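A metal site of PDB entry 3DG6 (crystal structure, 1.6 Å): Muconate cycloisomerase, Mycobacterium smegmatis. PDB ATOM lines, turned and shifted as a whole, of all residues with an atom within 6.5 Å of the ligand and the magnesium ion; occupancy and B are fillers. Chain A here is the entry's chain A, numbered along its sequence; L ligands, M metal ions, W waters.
Water W2 lies within hydrogen-bond range of OE2 of Glu 243 and OD1 of Asp 191. Water W3 bridges OE2 of Glu 243 (2.7 Å) and ND2 of Asn 193 (3.5 Å). Water W1 lies within hydrogen-bond range of the side-chain hydroxyl (OG1) of Thr 54 (2.8 Å), the side-chain hydroxyl (OG) of Ser 23 (2.9 Å) and the backbone carbonyl oxygen (O) of Phe 53 (3.4 Å).
CE1 of Phe 21 touches C3 of the ligand, at 3.7 Å. Arg 51 touches the ligand (CD to O3, 3.8 Å). CE1 of Phe 53 touches O3 of the ligand (3.9 Å). SD of Met 134 touches C6 of the ligand (3.5 Å). O of Asn 293 touches C6 of the ligand (3.3 Å). Ile 295 touches the ligand (CG1 to C5, 3.8 Å). Within 4 Å of the ligand: Phe 21, Arg 51, Phe 53, Thr 54, Met 134, Lys 160, Lys 162, Asp 191, Asn 193, Glu 217, Asp 242, Lys 266, Asn 293, Gln 294 and Ile 295. The nearest printed residue that does not touch the ligand is Glu 320 (4.1 Å).
The side-chain carboxylate (OE1) of Glu 217 lies within salt-bridge range of the side-chain amino group (NZ) of Lys 160. The side-chain carboxylate of Asp 191 sits close to the side-chain amino group of Lys 160 (3.1 Å). N of Asp 242 is in hydrogen-bond range of OE2 of Glu 218, 2.7 Å away. The side-chain amino group (NZ) of Lys 160 is in salt-bridge range of the side-chain carboxylate (OE1) of Glu 320, 2.7 Å away. The side-chain amino group (NZ) of Lys 162 sits at hydrogen-bond distance from the side-chain amide oxygen (OD1) of Asn 193 (2.8 Å). The backbone NH (N) of Asn 193 lies within hydrogen-bond range of the backbone carbonyl oxygen (O) of Glu 218. O of Glu 320 is in hydrogen-bond range of ND2 of Asn 293, at 2.9 Å. NH2 of Arg 51 lies within hydrogen-bond range of O of Ile 295, 2.9 Å away.
NZ of Lys 160 touches the magnesium ion (3.4 Å).
The side-chain carboxylate (OE2) of Glu 217 is bound to the magnesium ion. OD2 of Asp 191 is bound to the magnesium ion. O1 of the ligand is bound to the magnesium ion (2.2 Å). OD2 of Asp 242 is bound to the magnesium ion. Water W2 is bound to the magnesium ion, at 2.2 Å. The magnesium ion is bound by O2 of the ligand (2.3 Å).
The side-chain amino group (NZ) of Lys 160 sits close to an oxygen (O1) of the ligand, at 2.7 Å. The side-chain amino group (NZ) of Lys 266 lies close to an oxygen (O4) of the ligand, 3.1 Å away. The side-chain amide nitrogen of Asn 193 sits close to an oxygen (O2) of the ligand (2.9 Å). An oxygen (O3) of the ligand sits at hydrogen-bond distance from the side-chain amide nitrogen of Gln 294. OG1 of Thr 54 is in hydrogen-bond range of O3 of the ligand, at 3.0 Å. NZ of Lys 162 sits close to O2 of the ligand, 3.2 Å away.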
ATOM      1  N   LEU A  19      -7.305  34.550  23.200  1.00  0.00           N
ATOM      2  CA  LEU A  19      -6.992  33.145  22.952  1.00  0.00           C
ATOM      3  C   LEU A  19      -5.480  33.074  22.796  1.00  0.00           C
ATOM      4  O   LEU A  19      -4.900  33.725  21.919  1.00  0.00           O
ATOM      5  CB  LEU A  19      -7.663  32.658  21.664  1.00  0.00           C
ATOM      6  CG  LEU A  19      -7.506  31.154  21.377  1.00  0.00           C
ATOM      7  CD1 LEU A  19      -8.271  30.344  22.417  1.00  0.00           C
ATOM      8  CD2 LEU A  19      -8.027  30.841  19.980  1.00  0.00           C
ATOM      9  N   PHE A  21      -1.861  30.712  22.440  1.00  0.00           N
ATOM     10  CA  PHE A  21      -1.316  29.447  21.954  1.00  0.00           C
ATOM     11  C   PHE A  21       0.187  29.591  21.721  1.00  0.00           C
ATOM     12  O   PHE A  21       0.735  30.683  21.836  1.00  0.00           O
ATOM     13  CB  PHE A  21      -2.053  28.998  20.695  1.00  0.00           C
ATOM     14  CG  PHE A  21      -2.347  30.117  19.732  1.00  0.00           C
ATOM     15  CD1 PHE A  21      -1.488  30.379  18.675  1.00  0.00           C
ATOM     16  CD2 PHE A  21      -3.468  30.933  19.913  1.00  0.00           C
ATOM     17  CE1 PHE A  21      -1.738  31.450  17.802  1.00  0.00           C
ATOM     18  CE2 PHE A  21      -3.721  31.990  19.058  1.00  0.00           C
ATOM     19  CZ  PHE A  21      -2.862  32.253  18.001  1.00  0.00           C
ATOM     20  N   SER A  23       2.187  29.689  19.077  1.00  0.00           N
ATOM     21  CA  SER A  23       2.672  30.589  18.038  1.00  0.00           C
ATOM     22  C   SER A  23       2.242  32.055  18.141  1.00  0.00           C
ATOM     23  O   SER A  23       2.739  32.899  17.395  1.00  0.00           O
ATOM     24  CB  SER A  23       2.282  30.041  16.669  1.00  0.00           C
ATOM     25  OG  SER A  23       0.887  29.836  16.583  1.00  0.00           O
ATOM     26  N   ARG A  51      -3.298  36.461  10.045  1.00  0.00           N
ATOM     27  CA  ARG A  51      -2.589  35.672  11.042  1.00  0.00           C
ATOM     28  C   ARG A  51      -1.117  35.714  10.680  1.00  0.00           C
ATOM     29  O   ARG A  51      -0.587  34.797  10.036  1.00  0.00           O
ATOM     30  CB  ARG A  51      -3.118  34.229  11.022  1.00  0.00           C
ATOM     31  CG  ARG A  51      -4.622  34.121  11.316  1.00  0.00           C
ATOM     32  CD  ARG A  51      -4.909  34.412  12.783  1.00  0.00           C
ATOM     33  NE  ARG A  51      -6.338  34.430  13.107  1.00  0.00           N
ATOM     34  CZ  ARG A  51      -7.058  35.544  13.268  1.00  0.00           C
ATOM     35  NH1 ARG A  51      -6.481  36.734  13.123  1.00  0.00           N
ATOM     36  NH2 ARG A  51      -8.336  35.471  13.612  1.00  0.00           N
ATOM     37  N   PHE A  53       1.480  35.135  12.347  1.00  0.00           N
ATOM     38  CA  PHE A  53       2.212  34.014  12.929  1.00  0.00           C
ATOM     39  C   PHE A  53       1.850  32.675  12.289  1.00  0.00           C
ATOM     40  O   PHE A  53       2.311  31.629  12.743  1.00  0.00           O
ATOM     41  CB  PHE A  53       1.940  33.958  14.437  1.00  0.00           C
ATOM     42  CG  PHE A  53       0.499  34.169  14.796  1.00  0.00           C
ATOM     43  CD1 PHE A  53      -0.454  33.187  14.505  1.00  0.00           C
ATOM     44  CD2 PHE A  53       0.080  35.358  15.384  1.00  0.00           C
ATOM     45  CE1 PHE A  53      -1.801  33.403  14.789  1.00  0.00           C
ATOM     46  CE2 PHE A  53      -1.270  35.573  15.677  1.00  0.00           C
ATOM     47  CZ  PHE A  53      -2.211  34.596  15.380  1.00  0.00           C
ATOM     48  N   THR A  54       1.024  32.714  11.249  1.00  0.00           N
ATOM     49  CA  THR A  54       0.605  31.500  10.551  1.00  0.00           C
ATOM     50  C   THR A  54       0.871  31.606   9.051  1.00  0.00           C
ATOM     51  O   THR A  54       1.464  30.705   8.462  1.00  0.00           O
ATOM     52  CB  THR A  54      -0.898  31.232  10.759  1.00  0.00           C
ATOM     53  OG1 THR A  54      -1.166  31.114  12.160  1.00  0.00           O
ATOM     54  CG2 THR A  54      -1.314  29.935  10.056  1.00  0.00           C
ATOM     55  N   TYR A  55       0.447  32.721   8.451  1.00  0.00           N
ATOM     56  CA  TYR A  55       0.631  32.922   7.008  1.00  0.00           C
ATOM     57  C   TYR A  55       1.459  34.159   6.666  1.00  0.00           C
ATOM     58  O   TYR A  55       1.936  34.295   5.543  1.00  0.00           O
ATOM     59  CB  TYR A  55      -0.724  33.054   6.317  1.00  0.00           C
ATOM     60  CG  TYR A  55      -1.663  31.923   6.611  1.00  0.00           C
ATOM     61  CD1 TYR A  55      -1.322  30.606   6.316  1.00  0.00           C
ATOM     62  CD2 TYR A  55      -2.910  32.164   7.191  1.00  0.00           C
ATOM     63  CE1 TYR A  55      -2.189  29.553   6.596  1.00  0.00           C
ATOM     64  CE2 TYR A  55      -3.784  31.118   7.482  1.00  0.00           C
ATOM     65  CZ  TYR A  55      -3.413  29.822   7.179  1.00  0.00           C
ATOM     66  OH  TYR A  55      -4.277  28.791   7.465  1.00  0.00           O
ATOM     67  N   MET A 134     -11.527  24.731  20.671  1.00  0.00           N
ATOM     68  CA  MET A 134     -10.094  24.825  20.941  1.00  0.00           C
ATOM     69  C   MET A 134      -9.895  25.514  22.296  1.00  0.00           C
ATOM     70  O   MET A 134     -10.365  26.631  22.497  1.00  0.00           O
ATOM     71  CB  MET A 134      -9.386  25.633  19.849  1.00  0.00           C
ATOM     72  CG  MET A 134      -9.694  25.191  18.422  1.00  0.00           C
ATOM     73  SD  MET A 134      -8.592  25.918  17.176  1.00  0.00           S
ATOM     74  CE  MET A 134      -9.043  27.662  17.276  1.00  0.00           C
ATOM     75  N   LYS A 160     -10.042  20.370  21.485  1.00  0.00           N
ATOM     76  CA  LYS A 160      -8.678  20.329  20.974  1.00  0.00           C
ATOM     77  C   LYS A 160      -7.894  21.200  21.949  1.00  0.00           C
ATOM     78  O   LYS A 160      -8.073  22.415  21.988  1.00  0.00           O
ATOM     79  CB  LYS A 160      -8.576  20.902  19.558  1.00  0.00           C
ATOM     80  CG  LYS A 160      -7.142  20.854  19.015  1.00  0.00           C
ATOM     81  CD  LYS A 160      -7.034  21.152  17.524  1.00  0.00           C
ATOM     82  CE  LYS A 160      -6.999  22.638  17.217  1.00  0.00           C
ATOM     83  NZ  LYS A 160      -6.800  22.856  15.750  1.00  0.00           N
ATOM     84  N   LYS A 162      -4.795  23.198  23.375  1.00  0.00           N
ATOM     85  CA  LYS A 162      -3.603  23.890  22.893  1.00  0.00           C
ATOM     86  C   LYS A 162      -2.468  23.528  23.828  1.00  0.00           C
ATOM     87  O   LYS A 162      -2.575  23.679  25.048  1.00  0.00           O
ATOM     88  CB  LYS A 162      -3.809  25.413  22.921  1.00  0.00           C
ATOM     89  CG  LYS A 162      -4.723  25.946  21.836  1.00  0.00           C
ATOM     90  CD  LYS A 162      -4.166  25.669  20.462  1.00  0.00           C
ATOM     91  CE  LYS A 162      -5.008  26.297  19.377  1.00  0.00           C
ATOM     92  NZ  LYS A 162      -4.402  26.063  18.049  1.00  0.00           N
ATOM     93  N   ASP A 191      -2.995  20.234  19.921  1.00  0.00           N
ATOM     94  CA  ASP A 191      -2.377  21.061  18.878  1.00  0.00           C
ATOM     95  C   ASP A 191      -1.253  21.849  19.552  1.00  0.00           C
ATOM     96  O   ASP A 191      -1.499  22.651  20.461  1.00  0.00           O
ATOM     97  CB  ASP A 191      -3.413  22.031  18.304  1.00  0.00           C
ATOM     98  CG  ASP A 191      -2.897  22.790  17.085  1.00  0.00           C
ATOM     99  OD1 ASP A 191      -1.671  22.904  16.903  1.00  0.00           O
ATOM    100  OD2 ASP A 191      -3.738  23.304  16.310  1.00  0.00           O
ATOM    101  N   ASN A 193       0.958  23.891  17.870  1.00  0.00           N
ATOM    102  CA  ASN A 193       1.323  25.082  17.129  1.00  0.00           C
ATOM    103  C   ASN A 193       2.828  25.300  17.008  1.00  0.00           C
ATOM    104  O   ASN A 193       3.323  26.419  17.208  1.00  0.00           O
ATOM    105  CB  ASN A 193       0.669  26.331  17.736  1.00  0.00           C
ATOM    106  CG  ASN A 193      -0.816  26.391  17.460  1.00  0.00           C
ATOM    107  OD1 ASN A 193      -1.631  26.263  18.365  1.00  0.00           O
ATOM    108  ND2 ASN A 193      -1.167  26.593  16.193  1.00  0.00           N
ATOM    109  N   GLU A 217      -1.662  17.353  16.554  1.00  0.00           N
ATOM    110  CA  GLU A 217      -1.579  18.379  15.515  1.00  0.00           C
ATOM    111  C   GLU A 217      -0.393  19.331  15.684  1.00  0.00           C
ATOM    112  O   GLU A 217      -0.236  19.974  16.727  1.00  0.00           O
ATOM    113  CB  GLU A 217      -2.879  19.191  15.475  1.00  0.00           C
ATOM    114  CG  GLU A 217      -2.945  20.228  14.356  1.00  0.00           C
ATOM    115  CD  GLU A 217      -4.305  20.901  14.257  1.00  0.00           C
ATOM    116  OE1 GLU A 217      -5.300  20.271  14.645  1.00  0.00           O
ATOM    117  OE2 GLU A 217      -4.359  22.050  13.765  1.00  0.00           O
ATOM    118  N   GLU A 218       0.442  19.415  14.648  1.00  0.00           N
ATOM    119  CA  GLU A 218       1.596  20.313  14.624  1.00  0.00           C
ATOM    120  C   GLU A 218       2.309  20.438  15.981  1.00  0.00           C
ATOM    121  O   GLU A 218       2.554  21.556  16.452  1.00  0.00           O
ATOM    122  CB  GLU A 218       1.156  21.706  14.151  1.00  0.00           C
ATOM    123  CG  GLU A 218       0.568  21.762  12.744  1.00  0.00           C
ATOM    124  CD  GLU A 218       1.632  21.693  11.655  1.00  0.00           C
ATOM    125  OE1 GLU A 218       2.818  21.553  11.988  1.00  0.00           O
ATOM    126  OE2 GLU A 218       1.268  21.799  10.462  1.00  0.00           O
ATOM    127  N   ILE A 240      -1.923  15.527  12.413  1.00  0.00           N
ATOM    128  CA  ILE A 240      -2.519  16.558  11.578  1.00  0.00           C
ATOM    129  C   ILE A 240      -1.567  17.696  11.247  1.00  0.00           C
ATOM    130  O   ILE A 240      -0.978  18.313  12.137  1.00  0.00           O
ATOM    131  CB  ILE A 240      -3.764  17.169  12.256  1.00  0.00           C
ATOM    132  CG1 ILE A 240      -4.836  16.110  12.467  1.00  0.00           C
ATOM    133  CG2 ILE A 240      -4.304  18.324  11.412  1.00  0.00           C
ATOM    134  CD1 ILE A 240      -6.025  16.598  13.289  1.00  0.00           C
ATOM    135  N   ASP A 242      -1.282  21.409   9.686  1.00  0.00           N
ATOM    136  CA  ASP A 242      -2.165  22.569   9.609  1.00  0.00           C
ATOM    137  C   ASP A 242      -1.467  23.744   8.932  1.00  0.00           C
ATOM    138  O   ASP A 242      -1.571  23.916   7.709  1.00  0.00           O
ATOM    139  CB  ASP A 242      -2.612  22.929  11.037  1.00  0.00           C
ATOM    140  CG  ASP A 242      -3.505  24.155  11.109  1.00  0.00           C
ATOM    141  OD1 ASP A 242      -3.832  24.735  10.046  1.00  0.00           O
ATOM    142  OD2 ASP A 242      -3.895  24.542  12.229  1.00  0.00           O
ATOM    143  N   GLU A 243      -0.738  24.544   9.703  1.00  0.00           N
ATOM    144  CA  GLU A 243      -0.043  25.689   9.115  1.00  0.00           C
ATOM    145  C   GLU A 243       1.015  25.273   8.093  1.00  0.00           C
ATOM    146  O   GLU A 243       1.434  26.080   7.260  1.00  0.00           O
ATOM    147  CB  GLU A 243       0.595  26.565  10.204  1.00  0.00           C
ATOM    148  CG  GLU A 243       1.450  25.832  11.218  1.00  0.00           C
ATOM    149  CD  GLU A 243       0.697  25.538  12.507  1.00  0.00           C
ATOM    150  OE1 GLU A 243       1.258  25.789  13.593  1.00  0.00           O
ATOM    151  OE2 GLU A 243      -0.451  25.062  12.437  1.00  0.00           O
ATOM    152  N   SER A 264      -5.497  19.123   8.002  1.00  0.00           N
ATOM    153  CA  SER A 264      -6.460  20.095   8.493  1.00  0.00           C
ATOM    154  C   SER A 264      -6.939  20.893   7.295  1.00  0.00           C
ATOM    155  O   SER A 264      -6.131  21.347   6.487  1.00  0.00           O
ATOM    156  CB  SER A 264      -5.785  21.045   9.491  1.00  0.00           C
ATOM    157  OG  SER A 264      -6.507  22.269   9.609  1.00  0.00           O
ATOM    158  N   LYS A 266      -8.935  24.272   6.337  1.00  0.00           N
ATOM    159  CA  LYS A 266      -9.474  25.512   6.883  1.00  0.00           C
ATOM    160  C   LYS A 266      -9.948  26.381   5.734  1.00  0.00           C
ATOM    161  O   LYS A 266      -9.175  26.766   4.867  1.00  0.00           O
ATOM    162  CB  LYS A 266      -8.417  26.253   7.708  1.00  0.00           C
ATOM    163  CG  LYS A 266      -8.069  25.541   9.009  1.00  0.00           C
ATOM    164  CD  LYS A 266      -7.227  26.416   9.918  1.00  0.00           C
ATOM    165  CE  LYS A 266      -6.818  25.663  11.177  1.00  0.00           C
ATOM    166  NZ  LYS A 266      -6.015  26.515  12.090  1.00  0.00           N
ATOM    167  N   GLY A 292     -10.705  22.639  10.438  1.00  0.00           N
ATOM    168  CA  GLY A 292     -10.094  23.404  11.506  1.00  0.00           C
ATOM    169  C   GLY A 292     -10.636  24.816  11.679  1.00  0.00           C
ATOM    170  O   GLY A 292     -11.449  25.288  10.894  1.00  0.00           O
ATOM    171  N   ASN A 293     -10.150  25.481  12.717  1.00  0.00           N
ATOM    172  CA  ASN A 293     -10.570  26.844  13.039  1.00  0.00           C
ATOM    173  C   ASN A 293      -9.378  27.781  12.950  1.00  0.00           C
ATOM    174  O   ASN A 293      -8.312  27.499  13.492  1.00  0.00           O
ATOM    175  CB  ASN A 293     -11.160  26.863  14.457  1.00  0.00           C
ATOM    176  CG  ASN A 293     -11.941  28.135  14.747  1.00  0.00           C
ATOM    177  OD1 ASN A 293     -11.373  29.222  14.868  1.00  0.00           O
ATOM    178  ND2 ASN A 293     -13.257  27.999  14.863  1.00  0.00           N
ATOM    179  N   GLN A 294      -9.554  28.901  12.251  1.00  0.00           N
ATOM    180  CA  GLN A 294      -8.498  29.900  12.065  1.00  0.00           C
ATOM    181  C   GLN A 294      -8.730  31.034  13.068  1.00  0.00           C
ATOM    182  O   GLN A 294      -8.312  32.172  12.827  1.00  0.00           O
ATOM    183  CB  GLN A 294      -8.577  30.458  10.640  1.00  0.00           C
ATOM    184  CG  GLN A 294      -7.297  31.094  10.143  1.00  0.00           C
ATOM    185  CD  GLN A 294      -6.289  30.061   9.665  1.00  0.00           C
ATOM    186  OE1 GLN A 294      -6.427  29.491   8.580  1.00  0.00           O
ATOM    187  NE2 GLN A 294      -5.282  29.806  10.484  1.00  0.00           N
ATOM    188  N   ILE A 295      -9.369  30.699  14.183  1.00  0.00           N
ATOM    189  CA  ILE A 295      -9.743  31.681  15.204  1.00  0.00           C
ATOM    190  C   ILE A 295     -10.711  32.585  14.445  1.00  0.00           C
ATOM    191  O   ILE A 295     -10.597  33.814  14.434  1.00  0.00           O
ATOM    192  CB  ILE A 295      -8.545  32.474  15.742  1.00  0.00           C
ATOM    193  CG1 ILE A 295      -7.435  31.510  16.181  1.00  0.00           C
ATOM    194  CG2 ILE A 295      -8.971  33.305  16.951  1.00  0.00           C
ATOM    195  CD1 ILE A 295      -6.140  32.179  16.587  1.00  0.00           C
ATOM    196  N   GLU A 320     -14.028  22.265  14.057  1.00  0.00           N
ATOM    197  CA  GLU A 320     -13.663  23.299  15.023  1.00  0.00           C
ATOM    198  C   GLU A 320     -14.489  24.536  14.658  1.00  0.00           C
ATOM    199  O   GLU A 320     -14.082  25.378  13.860  1.00  0.00           O
ATOM    200  CB  GLU A 320     -12.155  23.524  14.947  1.00  0.00           C
ATOM    201  CG  GLU A 320     -11.408  22.317  15.495  1.00  0.00           C
ATOM    202  CD  GLU A 320      -9.957  22.219  15.087  1.00  0.00           C
ATOM    203  OE1 GLU A 320      -9.334  23.268  14.811  1.00  0.00           O
ATOM    204  OE2 GLU A 320      -9.437  21.081  15.059  1.00  0.00           O
HETATM  205  C1  LIG L   1      -4.974  26.008  14.939  1.00  0.00           C
HETATM  206  O1  LIG L   1      -5.669  25.044  14.544  1.00  0.00           O
HETATM  207  O2  LIG L   1      -3.731  26.072  14.893  1.00  0.00           O
HETATM  208  C2  LIG L   1      -3.779  28.940  15.796  1.00  0.00           C
HETATM  209  C3  LIG L   1      -3.244  29.740  14.870  1.00  0.00           C
HETATM  210  C4  LIG L   1      -4.098  29.841  13.857  1.00  0.00           C
HETATM  211  O3  LIG L   1      -4.019  30.702  12.975  1.00  0.00           O
HETATM  212  O4  LIG L   1      -5.072  28.885  13.885  1.00  0.00           O
HETATM  213  C5  LIG L   1      -5.192  28.634  15.286  1.00  0.00           C
HETATM  214  C6  LIG L   1      -5.748  27.205  15.582  1.00  0.00           C
HETATM  215 MG    MG M   1      -3.873  23.870  14.309  1.00  0.00          MG
HETATM  216  O   HOH W   1       0.060  29.320  13.895  1.00  0.00           O
HETATM  217  O   HOH W   2      -1.689  23.648  14.216  1.00  0.00           O
HETATM  218  O   HOH W   3      -1.918  27.345  12.878  1.00  0.00           O
